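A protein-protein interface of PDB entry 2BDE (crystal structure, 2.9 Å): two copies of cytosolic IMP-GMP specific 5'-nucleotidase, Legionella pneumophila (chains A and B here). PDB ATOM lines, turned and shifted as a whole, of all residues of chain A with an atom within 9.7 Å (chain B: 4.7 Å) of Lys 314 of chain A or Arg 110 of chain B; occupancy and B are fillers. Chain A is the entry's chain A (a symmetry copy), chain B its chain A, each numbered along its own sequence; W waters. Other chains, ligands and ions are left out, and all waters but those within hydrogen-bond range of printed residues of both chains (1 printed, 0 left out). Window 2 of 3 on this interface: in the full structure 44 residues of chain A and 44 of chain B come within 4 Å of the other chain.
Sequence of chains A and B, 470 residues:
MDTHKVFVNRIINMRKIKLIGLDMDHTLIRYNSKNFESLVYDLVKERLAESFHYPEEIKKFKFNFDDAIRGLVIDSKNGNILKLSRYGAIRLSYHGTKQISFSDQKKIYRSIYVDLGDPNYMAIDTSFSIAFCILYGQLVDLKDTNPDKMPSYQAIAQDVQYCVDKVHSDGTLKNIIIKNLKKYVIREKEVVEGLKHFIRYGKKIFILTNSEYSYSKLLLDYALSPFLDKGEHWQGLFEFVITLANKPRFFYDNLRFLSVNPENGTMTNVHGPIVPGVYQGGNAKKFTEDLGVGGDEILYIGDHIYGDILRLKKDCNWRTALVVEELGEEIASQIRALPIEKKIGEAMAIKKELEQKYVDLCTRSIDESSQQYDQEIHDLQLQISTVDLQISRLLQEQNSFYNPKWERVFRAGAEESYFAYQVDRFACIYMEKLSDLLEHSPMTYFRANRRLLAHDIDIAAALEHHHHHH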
ATOM      1  N   PHE A 251     -11.579  15.649  12.879  1.00  0.00           N
ATOM      2  CA  PHE A 251     -10.293  16.062  13.431  1.00  0.00           C
ATOM      3  C   PHE A 251      -9.183  16.379  12.451  1.00  0.00           C
ATOM      4  O   PHE A 251      -8.456  17.352  12.631  1.00  0.00           O
ATOM      5  CB  PHE A 251      -9.782  15.006  14.412  1.00  0.00           C
ATOM      6  CG  PHE A 251     -10.718  14.748  15.533  1.00  0.00           C
ATOM      7  CD1 PHE A 251     -11.523  13.606  15.536  1.00  0.00           C
ATOM      8  CD2 PHE A 251     -10.868  15.690  16.545  1.00  0.00           C
ATOM      9  CE1 PHE A 251     -12.475  13.406  16.525  1.00  0.00           C
ATOM     10  CE2 PHE A 251     -11.815  15.506  17.539  1.00  0.00           C
ATOM     11  CZ  PHE A 251     -12.628  14.359  17.532  1.00  0.00           C
ATOM     12  N   TYR A 252      -9.037  15.569  11.413  1.00  0.00           N
ATOM     13  CA  TYR A 252      -7.949  15.812  10.488  1.00  0.00           C
ATOM     14  C   TYR A 252      -8.351  16.279   9.096  1.00  0.00           C
ATOM     15  O   TYR A 252      -7.509  16.756   8.344  1.00  0.00           O
ATOM     16  CB  TYR A 252      -7.076  14.555  10.393  1.00  0.00           C
ATOM     17  CG  TYR A 252      -7.851  13.311  10.024  1.00  0.00           C
ATOM     18  CD1 TYR A 252      -8.188  12.352  10.987  1.00  0.00           C
ATOM     19  CD2 TYR A 252      -8.286  13.111   8.711  1.00  0.00           C
ATOM     20  CE1 TYR A 252      -8.945  11.222  10.640  1.00  0.00           C
ATOM     21  CE2 TYR A 252      -9.040  12.001   8.361  1.00  0.00           C
ATOM     22  CZ  TYR A 252      -9.367  11.061   9.322  1.00  0.00           C
ATOM     23  OH  TYR A 252     -10.127   9.975   8.947  1.00  0.00           O
ATOM     24  N   LYS A 285      -9.375  21.995  12.559  1.00  0.00           N
ATOM     25  CA  LYS A 285      -8.472  23.049  12.119  1.00  0.00           C
ATOM     26  C   LYS A 285      -9.149  24.422  12.207  1.00  0.00           C
ATOM     27  O   LYS A 285      -8.661  25.306  12.920  1.00  0.00           O
ATOM     28  CB  LYS A 285      -7.994  22.756  10.689  1.00  0.00           C
ATOM     29  CG  LYS A 285      -7.175  23.855  10.014  1.00  0.00           C
ATOM     30  CD  LYS A 285      -5.869  24.152  10.731  1.00  0.00           C
ATOM     31  CE  LYS A 285      -4.682  23.457  10.077  1.00  0.00           C
ATOM     32  NZ  LYS A 285      -4.756  21.975  10.202  1.00  0.00           N
ATOM     33  N   ASP A 308      -7.510   5.920  12.826  1.00  0.00           N
ATOM     34  CA  ASP A 308      -6.080   5.580  12.814  1.00  0.00           C
ATOM     35  C   ASP A 308      -5.338   6.511  13.762  1.00  0.00           C
ATOM     36  O   ASP A 308      -5.251   7.712  13.513  1.00  0.00           O
ATOM     37  CB  ASP A 308      -5.505   5.747  11.402  1.00  0.00           C
ATOM     38  CG  ASP A 308      -3.993   5.618  11.369  1.00  0.00           C
ATOM     39  OD1 ASP A 308      -3.475   4.588  11.866  1.00  0.00           O
ATOM     40  OD2 ASP A 308      -3.316   6.543  10.855  1.00  0.00           O
ATOM     41  N   ILE A 309      -4.784   5.952  14.831  1.00  0.00           N
ATOM     42  CA  ILE A 309      -4.082   6.749  15.826  1.00  0.00           C
ATOM     43  C   ILE A 309      -3.001   7.663  15.274  1.00  0.00           C
ATOM     44  O   ILE A 309      -2.883   8.819  15.696  1.00  0.00           O
ATOM     45  CB  ILE A 309      -3.465   5.855  16.914  1.00  0.00           C
ATOM     46  CG1 ILE A 309      -4.569   5.028  17.572  1.00  0.00           C
ATOM     47  CG2 ILE A 309      -2.762   6.703  17.954  1.00  0.00           C
ATOM     48  CD1 ILE A 309      -4.104   4.178  18.703  1.00  0.00           C
ATOM     49  N   LEU A 310      -2.225   7.163  14.319  1.00  0.00           N
ATOM     50  CA  LEU A 310      -1.144   7.958  13.742  1.00  0.00           C
ATOM     51  C   LEU A 310      -1.630   9.230  13.071  1.00  0.00           C
ATOM     52  O   LEU A 310      -1.085  10.306  13.294  1.00  0.00           O
ATOM     53  CB  LEU A 310      -0.336   7.119  12.742  1.00  0.00           C
ATOM     54  CG  LEU A 310       0.898   7.775  12.082  1.00  0.00           C
ATOM     55  CD1 LEU A 310       0.493   8.482  10.789  1.00  0.00           C
ATOM     56  CD2 LEU A 310       1.564   8.745  13.063  1.00  0.00           C
ATOM     57  N   ARG A 311      -2.647   9.107  12.239  1.00  0.00           N
ATOM     58  CA  ARG A 311      -3.161  10.280  11.572  1.00  0.00           C
ATOM     59  C   ARG A 311      -3.897  11.170  12.557  1.00  0.00           C
ATOM     60  O   ARG A 311      -3.756  12.387  12.521  1.00  0.00           O
ATOM     61  CB  ARG A 311      -4.085   9.872  10.438  1.00  0.00           C
ATOM     62  CG  ARG A 311      -4.695  11.037   9.706  1.00  0.00           C
ATOM     63  CD  ARG A 311      -5.176  10.566   8.361  1.00  0.00           C
ATOM     64  NE  ARG A 311      -5.828   9.272   8.498  1.00  0.00           N
ATOM     65  CZ  ARG A 311      -6.419   8.633   7.498  1.00  0.00           C
ATOM     66  NH1 ARG A 311      -6.433   9.178   6.284  1.00  0.00           N
ATOM     67  NH2 ARG A 311      -7.000   7.456   7.713  1.00  0.00           N
ATOM     68  N   LEU A 312      -4.683  10.566  13.440  1.00  0.00           N
ATOM     69  CA  LEU A 312      -5.422  11.341  14.426  1.00  0.00           C
ATOM     70  C   LEU A 312      -4.505  12.206  15.283  1.00  0.00           C
ATOM     71  O   LEU A 312      -4.817  13.363  15.563  1.00  0.00           O
ATOM     72  CB  LEU A 312      -6.242  10.425  15.343  1.00  0.00           C
ATOM     73  CG  LEU A 312      -7.559   9.837  14.829  1.00  0.00           C
ATOM     74  CD1 LEU A 312      -8.019   8.709  15.735  1.00  0.00           C
ATOM     75  CD2 LEU A 312      -8.591  10.918  14.742  1.00  0.00           C
ATOM     76  N   LYS A 313      -3.369  11.653  15.699  1.00  0.00           N
ATOM     77  CA  LYS A 313      -2.445  12.400  16.548  1.00  0.00           C
ATOM     78  C   LYS A 313      -1.501  13.357  15.824  1.00  0.00           C
ATOM     79  O   LYS A 313      -1.141  14.396  16.377  1.00  0.00           O
ATOM     80  CB  LYS A 313      -1.616  11.433  17.394  1.00  0.00           C
ATOM     81  CG  LYS A 313      -2.438  10.596  18.342  1.00  0.00           C
ATOM     82  CD  LYS A 313      -3.328  11.466  19.209  1.00  0.00           C
ATOM     83  CE  LYS A 313      -2.532  12.327  20.157  1.00  0.00           C
ATOM     84  NZ  LYS A 313      -3.424  13.264  20.879  1.00  0.00           N
ATOM     85  N   LYS A 314      -1.100  13.004  14.602  1.00  0.00           N
ATOM     86  CA  LYS A 314      -0.185  13.832  13.819  1.00  0.00           C
ATOM     87  C   LYS A 314      -0.898  14.904  13.023  1.00  0.00           C
ATOM     88  O   LYS A 314      -0.358  15.985  12.785  1.00  0.00           O
ATOM     89  CB  LYS A 314       0.626  12.969  12.847  1.00  0.00           C
ATOM     90  CG  LYS A 314       1.579  13.778  11.967  1.00  0.00           C
ATOM     91  CD  LYS A 314       2.566  12.887  11.207  1.00  0.00           C
ATOM     92  CE  LYS A 314       1.926  12.163  10.014  1.00  0.00           C
ATOM     93  NZ  LYS A 314       1.594  13.095   8.892  1.00  0.00           N
ATOM     94  N   ASP A 315      -2.116  14.601  12.607  1.00  0.00           N
ATOM     95  CA  ASP A 315      -2.869  15.544  11.817  1.00  0.00           C
ATOM     96  C   ASP A 315      -3.797  16.424  12.622  1.00  0.00           C
ATOM     97  O   ASP A 315      -4.250  17.443  12.107  1.00  0.00           O
ATOM     98  CB  ASP A 315      -3.643  14.802  10.733  1.00  0.00           C
ATOM     99  CG  ASP A 315      -2.719  14.100   9.745  1.00  0.00           C
ATOM    100  OD1 ASP A 315      -3.234  13.379   8.859  1.00  0.00           O
ATOM    101  OD2 ASP A 315      -1.475  14.277   9.854  1.00  0.00           O
ATOM    102  N   CYS A 316      -4.083  16.076  13.877  1.00  0.00           N
ATOM    103  CA  CYS A 316      -4.985  16.937  14.627  1.00  0.00           C
ATOM    104  C   CYS A 316      -4.268  17.976  15.460  1.00  0.00           C
ATOM    105  O   CYS A 316      -4.489  19.167  15.252  1.00  0.00           O
ATOM    106  CB  CYS A 316      -5.931  16.149  15.516  1.00  0.00           C
ATOM    107  SG  CYS A 316      -7.170  17.249  16.207  1.00  0.00           S
ATOM    108  N   ASN A 317      -3.446  17.530  16.409  1.00  0.00           N
ATOM    109  CA  ASN A 317      -2.645  18.416  17.260  1.00  0.00           C
ATOM    110  C   ASN A 317      -3.214  18.854  18.586  1.00  0.00           C
ATOM    111  O   ASN A 317      -2.527  19.525  19.356  1.00  0.00           O
ATOM    112  CB  ASN A 317      -2.160  19.650  16.473  1.00  0.00           C
ATOM    113  CG  ASN A 317      -2.731  20.974  16.991  1.00  0.00           C
ATOM    114  OD1 ASN A 317      -1.980  21.834  17.450  1.00  0.00           O
ATOM    115  ND2 ASN A 317      -4.051  21.151  16.895  1.00  0.00           N
ATOM    116  N   TRP A 318      -4.451  18.514  18.897  1.00  0.00           N
ATOM    117  CA  TRP A 318      -4.881  18.928  20.215  1.00  0.00           C
ATOM    118  C   TRP A 318      -5.018  17.732  21.166  1.00  0.00           C
ATOM    119  O   TRP A 318      -5.232  16.606  20.729  1.00  0.00           O
ATOM    120  CB  TRP A 318      -6.127  19.808  20.119  1.00  0.00           C
ATOM    121  CG  TRP A 318      -7.345  19.200  19.629  1.00  0.00           C
ATOM    122  CD1 TRP A 318      -7.759  17.940  19.859  1.00  0.00           C
ATOM    123  CD2 TRP A 318      -8.463  19.896  19.060  1.00  0.00           C
ATOM    124  NE1 TRP A 318      -9.087  17.790  19.494  1.00  0.00           N
ATOM    125  CE2 TRP A 318      -9.544  18.983  19.005  1.00  0.00           C
ATOM    126  CE3 TRP A 318      -8.660  21.201  18.600  1.00  0.00           C
ATOM    127  CZ2 TRP A 318     -10.808  19.329  18.530  1.00  0.00           C
ATOM    128  CZ3 TRP A 318      -9.928  21.549  18.120  1.00  0.00           C
ATOM    129  CH2 TRP A 318     -10.983  20.610  18.093  1.00  0.00           C
ATOM    130  N   THR A 320      -5.880  14.730  23.676  1.00  0.00           N
ATOM    131  CA  THR A 320      -6.962  13.761  23.661  1.00  0.00           C
ATOM    132  C   THR A 320      -6.955  12.776  24.827  1.00  0.00           C
ATOM    133  O   THR A 320      -5.921  12.186  25.165  1.00  0.00           O
ATOM    134  CB  THR A 320      -6.963  12.967  22.332  1.00  0.00           C
ATOM    135  OG1 THR A 320      -5.654  12.443  22.076  1.00  0.00           O
ATOM    136  CG2 THR A 320      -7.393  13.871  21.180  1.00  0.00           C
ATOM    137  N   ARG A 425      -0.977   5.107  23.429  1.00  0.00           N
ATOM    138  CA  ARG A 425      -0.537   6.006  22.384  1.00  0.00           C
ATOM    139  C   ARG A 425      -1.523   7.121  22.123  1.00  0.00           C
ATOM    140  O   ARG A 425      -1.139   8.273  21.909  1.00  0.00           O
ATOM    141  CB  ARG A 425      -0.318   5.222  21.091  1.00  0.00           C
ATOM    142  CG  ARG A 425       0.421   5.969  20.001  1.00  0.00           C
ATOM    143  CD  ARG A 425       0.337   5.192  18.708  1.00  0.00           C
ATOM    144  NE  ARG A 425       1.621   5.066  18.018  1.00  0.00           N
ATOM    145  CZ  ARG A 425       2.298   6.078  17.480  1.00  0.00           C
ATOM    146  NH1 ARG A 425       1.820   7.323  17.546  1.00  0.00           N
ATOM    147  NH2 ARG A 425       3.453   5.838  16.866  1.00  0.00           N
ATOM    148  N   PHE A 426      -2.803   6.797  22.163  1.00  0.00           N
ATOM    149  CA  PHE A 426      -3.787   7.812  21.840  1.00  0.00           C
ATOM    150  C   PHE A 426      -4.232   8.781  22.924  1.00  0.00           C
ATOM    151  O   PHE A 426      -4.390   9.980  22.660  1.00  0.00           O
ATOM    152  CB  PHE A 426      -5.010   7.145  21.218  1.00  0.00           C
ATOM    153  CG  PHE A 426      -6.151   8.074  20.997  1.00  0.00           C
ATOM    154  CD1 PHE A 426      -7.135   8.228  21.971  1.00  0.00           C
ATOM    155  CD2 PHE A 426      -6.242   8.801  19.820  1.00  0.00           C
ATOM    156  CE1 PHE A 426      -8.205   9.100  21.774  1.00  0.00           C
ATOM    157  CE2 PHE A 426      -7.305   9.677  19.608  1.00  0.00           C
ATOM    158  CZ  PHE A 426      -8.291   9.825  20.591  1.00  0.00           C
ATOM    159  N   GLN B 105      10.398  24.044  15.067  1.00  0.00           N
ATOM    160  CA  GLN B 105      10.210  22.629  14.794  1.00  0.00           C
ATOM    161  C   GLN B 105       8.747  22.372  14.464  1.00  0.00           C
ATOM    162  O   GLN B 105       8.423  21.749  13.448  1.00  0.00           O
ATOM    163  CB  GLN B 105      10.607  21.796  16.006  1.00  0.00           C
ATOM    164  CG  GLN B 105      10.312  20.328  15.816  1.00  0.00           C
ATOM    165  CD  GLN B 105       9.604  19.738  17.011  1.00  0.00           C
ATOM    166  OE1 GLN B 105      10.181  19.622  18.101  1.00  0.00           O
ATOM    167  NE2 GLN B 105       8.333  19.375  16.823  1.00  0.00           N
ATOM    168  N   LYS B 106       7.880  22.865  15.344  1.00  0.00           N
ATOM    169  CA  LYS B 106       6.437  22.726  15.203  1.00  0.00           C
ATOM    170  C   LYS B 106       5.991  23.272  13.839  1.00  0.00           C
ATOM    171  O   LYS B 106       5.246  22.607  13.117  1.00  0.00           O
ATOM    172  CB  LYS B 106       5.727  23.480  16.350  1.00  0.00           C
ATOM    173  CG  LYS B 106       4.706  22.658  17.191  1.00  0.00           C
ATOM    174  CD  LYS B 106       3.373  22.430  16.425  1.00  0.00           C
ATOM    175  CE  LYS B 106       2.330  21.603  17.194  1.00  0.00           C
ATOM    176  NZ  LYS B 106       1.158  21.349  16.344  1.00  0.00           N
ATOM    177  N   LYS B 107       6.460  24.461  13.469  1.00  0.00           N
ATOM    178  CA  LYS B 107       6.058  25.045  12.191  1.00  0.00           C
ATOM    179  C   LYS B 107       6.607  24.288  10.978  1.00  0.00           C
ATOM    180  O   LYS B 107       5.999  24.316   9.900  1.00  0.00           O
ATOM    181  CB  LYS B 107       6.472  26.519  12.110  1.00  0.00           C
ATOM    182  CG  LYS B 107       7.963  26.767  12.175  1.00  0.00           C
ATOM    183  CD  LYS B 107       8.466  27.610  10.998  1.00  0.00           C
ATOM    184  CE  LYS B 107       8.358  26.868   9.663  1.00  0.00           C
ATOM    185  NZ  LYS B 107       9.031  27.603   8.543  1.00  0.00           N
ATOM    186  N   ILE B 108       7.743  23.610  11.165  1.00  0.00           N
ATOM    187  CA  ILE B 108       8.408  22.825  10.119  1.00  0.00           C
ATOM    188  C   ILE B 108       7.722  21.481   9.889  1.00  0.00           C
ATOM    189  O   ILE B 108       7.502  21.072   8.750  1.00  0.00           O
ATOM    190  CB  ILE B 108       9.870  22.525  10.502  1.00  0.00           C
ATOM    191  CG1 ILE B 108      10.669  23.814  10.575  1.00  0.00           C
ATOM    192  CG2 ILE B 108      10.502  21.575   9.495  1.00  0.00           C
ATOM    193  CD1 ILE B 108      12.035  23.614  11.183  1.00  0.00           C
ATOM    194  N   TYR B 109       7.406  20.792  10.982  1.00  0.00           N
ATOM    195  CA  TYR B 109       6.756  19.495  10.891  1.00  0.00           C
ATOM    196  C   TYR B 109       5.238  19.558  11.108  1.00  0.00           C
ATOM    197  O   TYR B 109       4.576  18.525  11.171  1.00  0.00           O
ATOM    198  CB  TYR B 109       7.394  18.500  11.887  1.00  0.00           C
ATOM    199  CG  TYR B 109       8.855  18.192  11.622  1.00  0.00           C
ATOM    200  CD1 TYR B 109       9.870  18.916  12.262  1.00  0.00           C
ATOM    201  CD2 TYR B 109       9.223  17.254  10.652  1.00  0.00           C
ATOM    202  CE1 TYR B 109      11.218  18.722  11.928  1.00  0.00           C
ATOM    203  CE2 TYR B 109      10.563  17.053  10.309  1.00  0.00           C
ATOM    204  CZ  TYR B 109      11.556  17.791  10.940  1.00  0.00           C
ATOM    205  OH  TYR B 109      12.869  17.634  10.531  1.00  0.00           O
ATOM    206  N   ARG B 110       4.690  20.762  11.228  1.00  0.00           N
ATOM    207  CA  ARG B 110       3.246  20.926  11.426  1.00  0.00           C
ATOM    208  C   ARG B 110       2.704  19.879  12.409  1.00  0.00           C
ATOM    209  O   ARG B 110       1.584  19.393  12.259  1.00  0.00           O
ATOM    210  CB  ARG B 110       2.495  20.782  10.091  1.00  0.00           C
ATOM    211  CG  ARG B 110       3.011  21.602   8.906  1.00  0.00           C
ATOM    212  CD  ARG B 110       2.194  21.229   7.660  1.00  0.00           C
ATOM    213  NE  ARG B 110       2.872  21.437   6.371  1.00  0.00           N
ATOM    214  CZ  ARG B 110       3.116  22.623   5.811  1.00  0.00           C
ATOM    215  NH1 ARG B 110       2.749  23.745   6.421  1.00  0.00           N
ATOM    216  NH2 ARG B 110       3.707  22.690   4.620  1.00  0.00           N
ATOM    217  N   SER B 111       3.499  19.537  13.414  1.00  0.00           N
ATOM    218  CA  SER B 111       3.099  18.537  14.395  1.00  0.00           C
ATOM    219  C   SER B 111       4.308  18.200  15.240  1.00  0.00           C
ATOM    220  O   SER B 111       5.438  18.452  14.838  1.00  0.00           O
ATOM    221  CB  SER B 111       2.617  17.267  13.683  1.00  0.00           C
ATOM    222  OG  SER B 111       2.276  16.240  14.604  1.00  0.00           O
ATOM    223  N   TYR B 113       4.845  15.171  16.024  1.00  0.00           N
ATOM    224  CA  TYR B 113       5.125  13.788  15.617  1.00  0.00           C
ATOM    225  C   TYR B 113       5.638  13.732  14.183  1.00  0.00           C
ATOM    226  O   TYR B 113       5.604  14.731  13.471  1.00  0.00           O
ATOM    227  CB  TYR B 113       3.859  12.913  15.695  1.00  0.00           C
ATOM    228  CG  TYR B 113       3.284  12.721  17.074  1.00  0.00           C
ATOM    229  CD1 TYR B 113       2.281  13.563  17.554  1.00  0.00           C
ATOM    230  CD2 TYR B 113       3.756  11.704  17.911  1.00  0.00           C
ATOM    231  CE1 TYR B 113       1.755  13.402  18.839  1.00  0.00           C
ATOM    232  CE2 TYR B 113       3.243  11.535  19.200  1.00  0.00           C
ATOM    233  CZ  TYR B 113       2.242  12.393  19.659  1.00  0.00           C
ATOM    234  OH  TYR B 113       1.757  12.268  20.944  1.00  0.00           O
ATOM    235  N   VAL B 114       6.112  12.559  13.768  1.00  0.00           N
ATOM    236  CA  VAL B 114       6.589  12.360  12.400  1.00  0.00           C
ATOM    237  C   VAL B 114       6.150  10.971  11.966  1.00  0.00           C
ATOM    238  O   VAL B 114       5.793  10.156  12.804  1.00  0.00           O
ATOM    239  CB  VAL B 114       8.136  12.472  12.269  1.00  0.00           C
ATOM    240  CG1 VAL B 114       8.607  13.868  12.676  1.00  0.00           C
ATOM    241  CG2 VAL B 114       8.813  11.407  13.106  1.00  0.00           C
ATOM    242  N   ASP B 115       6.186  10.708  10.662  1.00  0.00           N
ATOM    243  CA  ASP B 115       5.754   9.431  10.090  1.00  0.00           C
ATOM    244  C   ASP B 115       6.951   8.629   9.581  1.00  0.00           C
ATOM    245  O   ASP B 115       7.403   8.814   8.444  1.00  0.00           O
ATOM    246  CB  ASP B 115       4.795   9.718   8.933  1.00  0.00           C
ATOM    247  CG  ASP B 115       4.066   8.486   8.438  1.00  0.00           C
ATOM    248  OD1 ASP B 115       4.643   7.375   8.450  1.00  0.00           O
ATOM    249  OD2 ASP B 115       2.899   8.640   8.009  1.00  0.00           O
HETATM  250  O   HOH W   1      -0.802  18.951  13.987  1.00  0.00           O
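N of Tyr 113 of chain B sits at hydrogen-bond distance from OG of Ser 111 of chain B, 3.1 Å away. The side-chain hydroxyl of Thr 320 of chain A sits at hydrogen-bond distance from the side-chain amino group of Lys 313 of chain A (2.7 Å). The side-chain carboxylate (OD2) of Asp 315 of chain A lies within salt-bridge range of the side-chain amino group (NZ) of Lys 314 of chain A, at 3.4 Å.
Among the printed residues, merely in contact across the chains: Leu 310 of chain A with Asp 115 of chain B, Lys 313 of chain A with Tyr 113 of chain B, Lys 314 of chain A with Arg 110 of chain B and Lys 314 of chain A with Asp 115 of chain B.
Water W1 lies within hydrogen-bond range of O of Arg 110 of chain B (3.0 Å) and O of Lys 314 of chain A (3.2 Å).
The side-chain amide oxygen (OD1) of Asn 317 of chain A lies within hydrogen-bond range of the side-chain amino group (NZ) of Lys 106 of chain B, at 3.4 Å. The side-chain hydroxyl (OG) of Ser 111 of chain B sits at hydrogen-bond distance from the backbone carbonyl oxygen (O) of Lys 314 of chain A (3.2 Å).
Lys 314 of chain A touches three residues of chain B. Ser 111 of chain B touches just one residue of chain A: Lys 314 (3.2 Å). Printed residues of chain A within 4 Å of Tyr 113 of chain B: Lys 313 (3.7 Å). Of the printed residues of chain A, Asp 115 of chain B touches Leu 310 and Lys 314. Lys 285 of chain A touches none of the printed residues of chain B. The nearest residue of chain A that does not touch Arg 110 of chain B is Asn 317 of chain A (5.6 Å).
No position is printed for both chains. Of the 6 pairs that touch across the chains among the printed residues, none has its exchanged pair printed and touching as well.
Printed residues of chain B that touch a printed residue of chain A: Lys 106, Arg 110, Ser 111, Tyr 113 and Asp 115. Of the 17 printed residues of chain A, 4 touch a printed residue of chain B. Hydrophobic or aromatic side chains of chain A that line the printed part of chain B: Leu 310. Among the printed residues, 6 pairs touch across the chains. Among the printed residues, no Asp or Glu carboxylate lies within 4 Å of a Lys or Arg side-chain nitrogen of the other chain.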
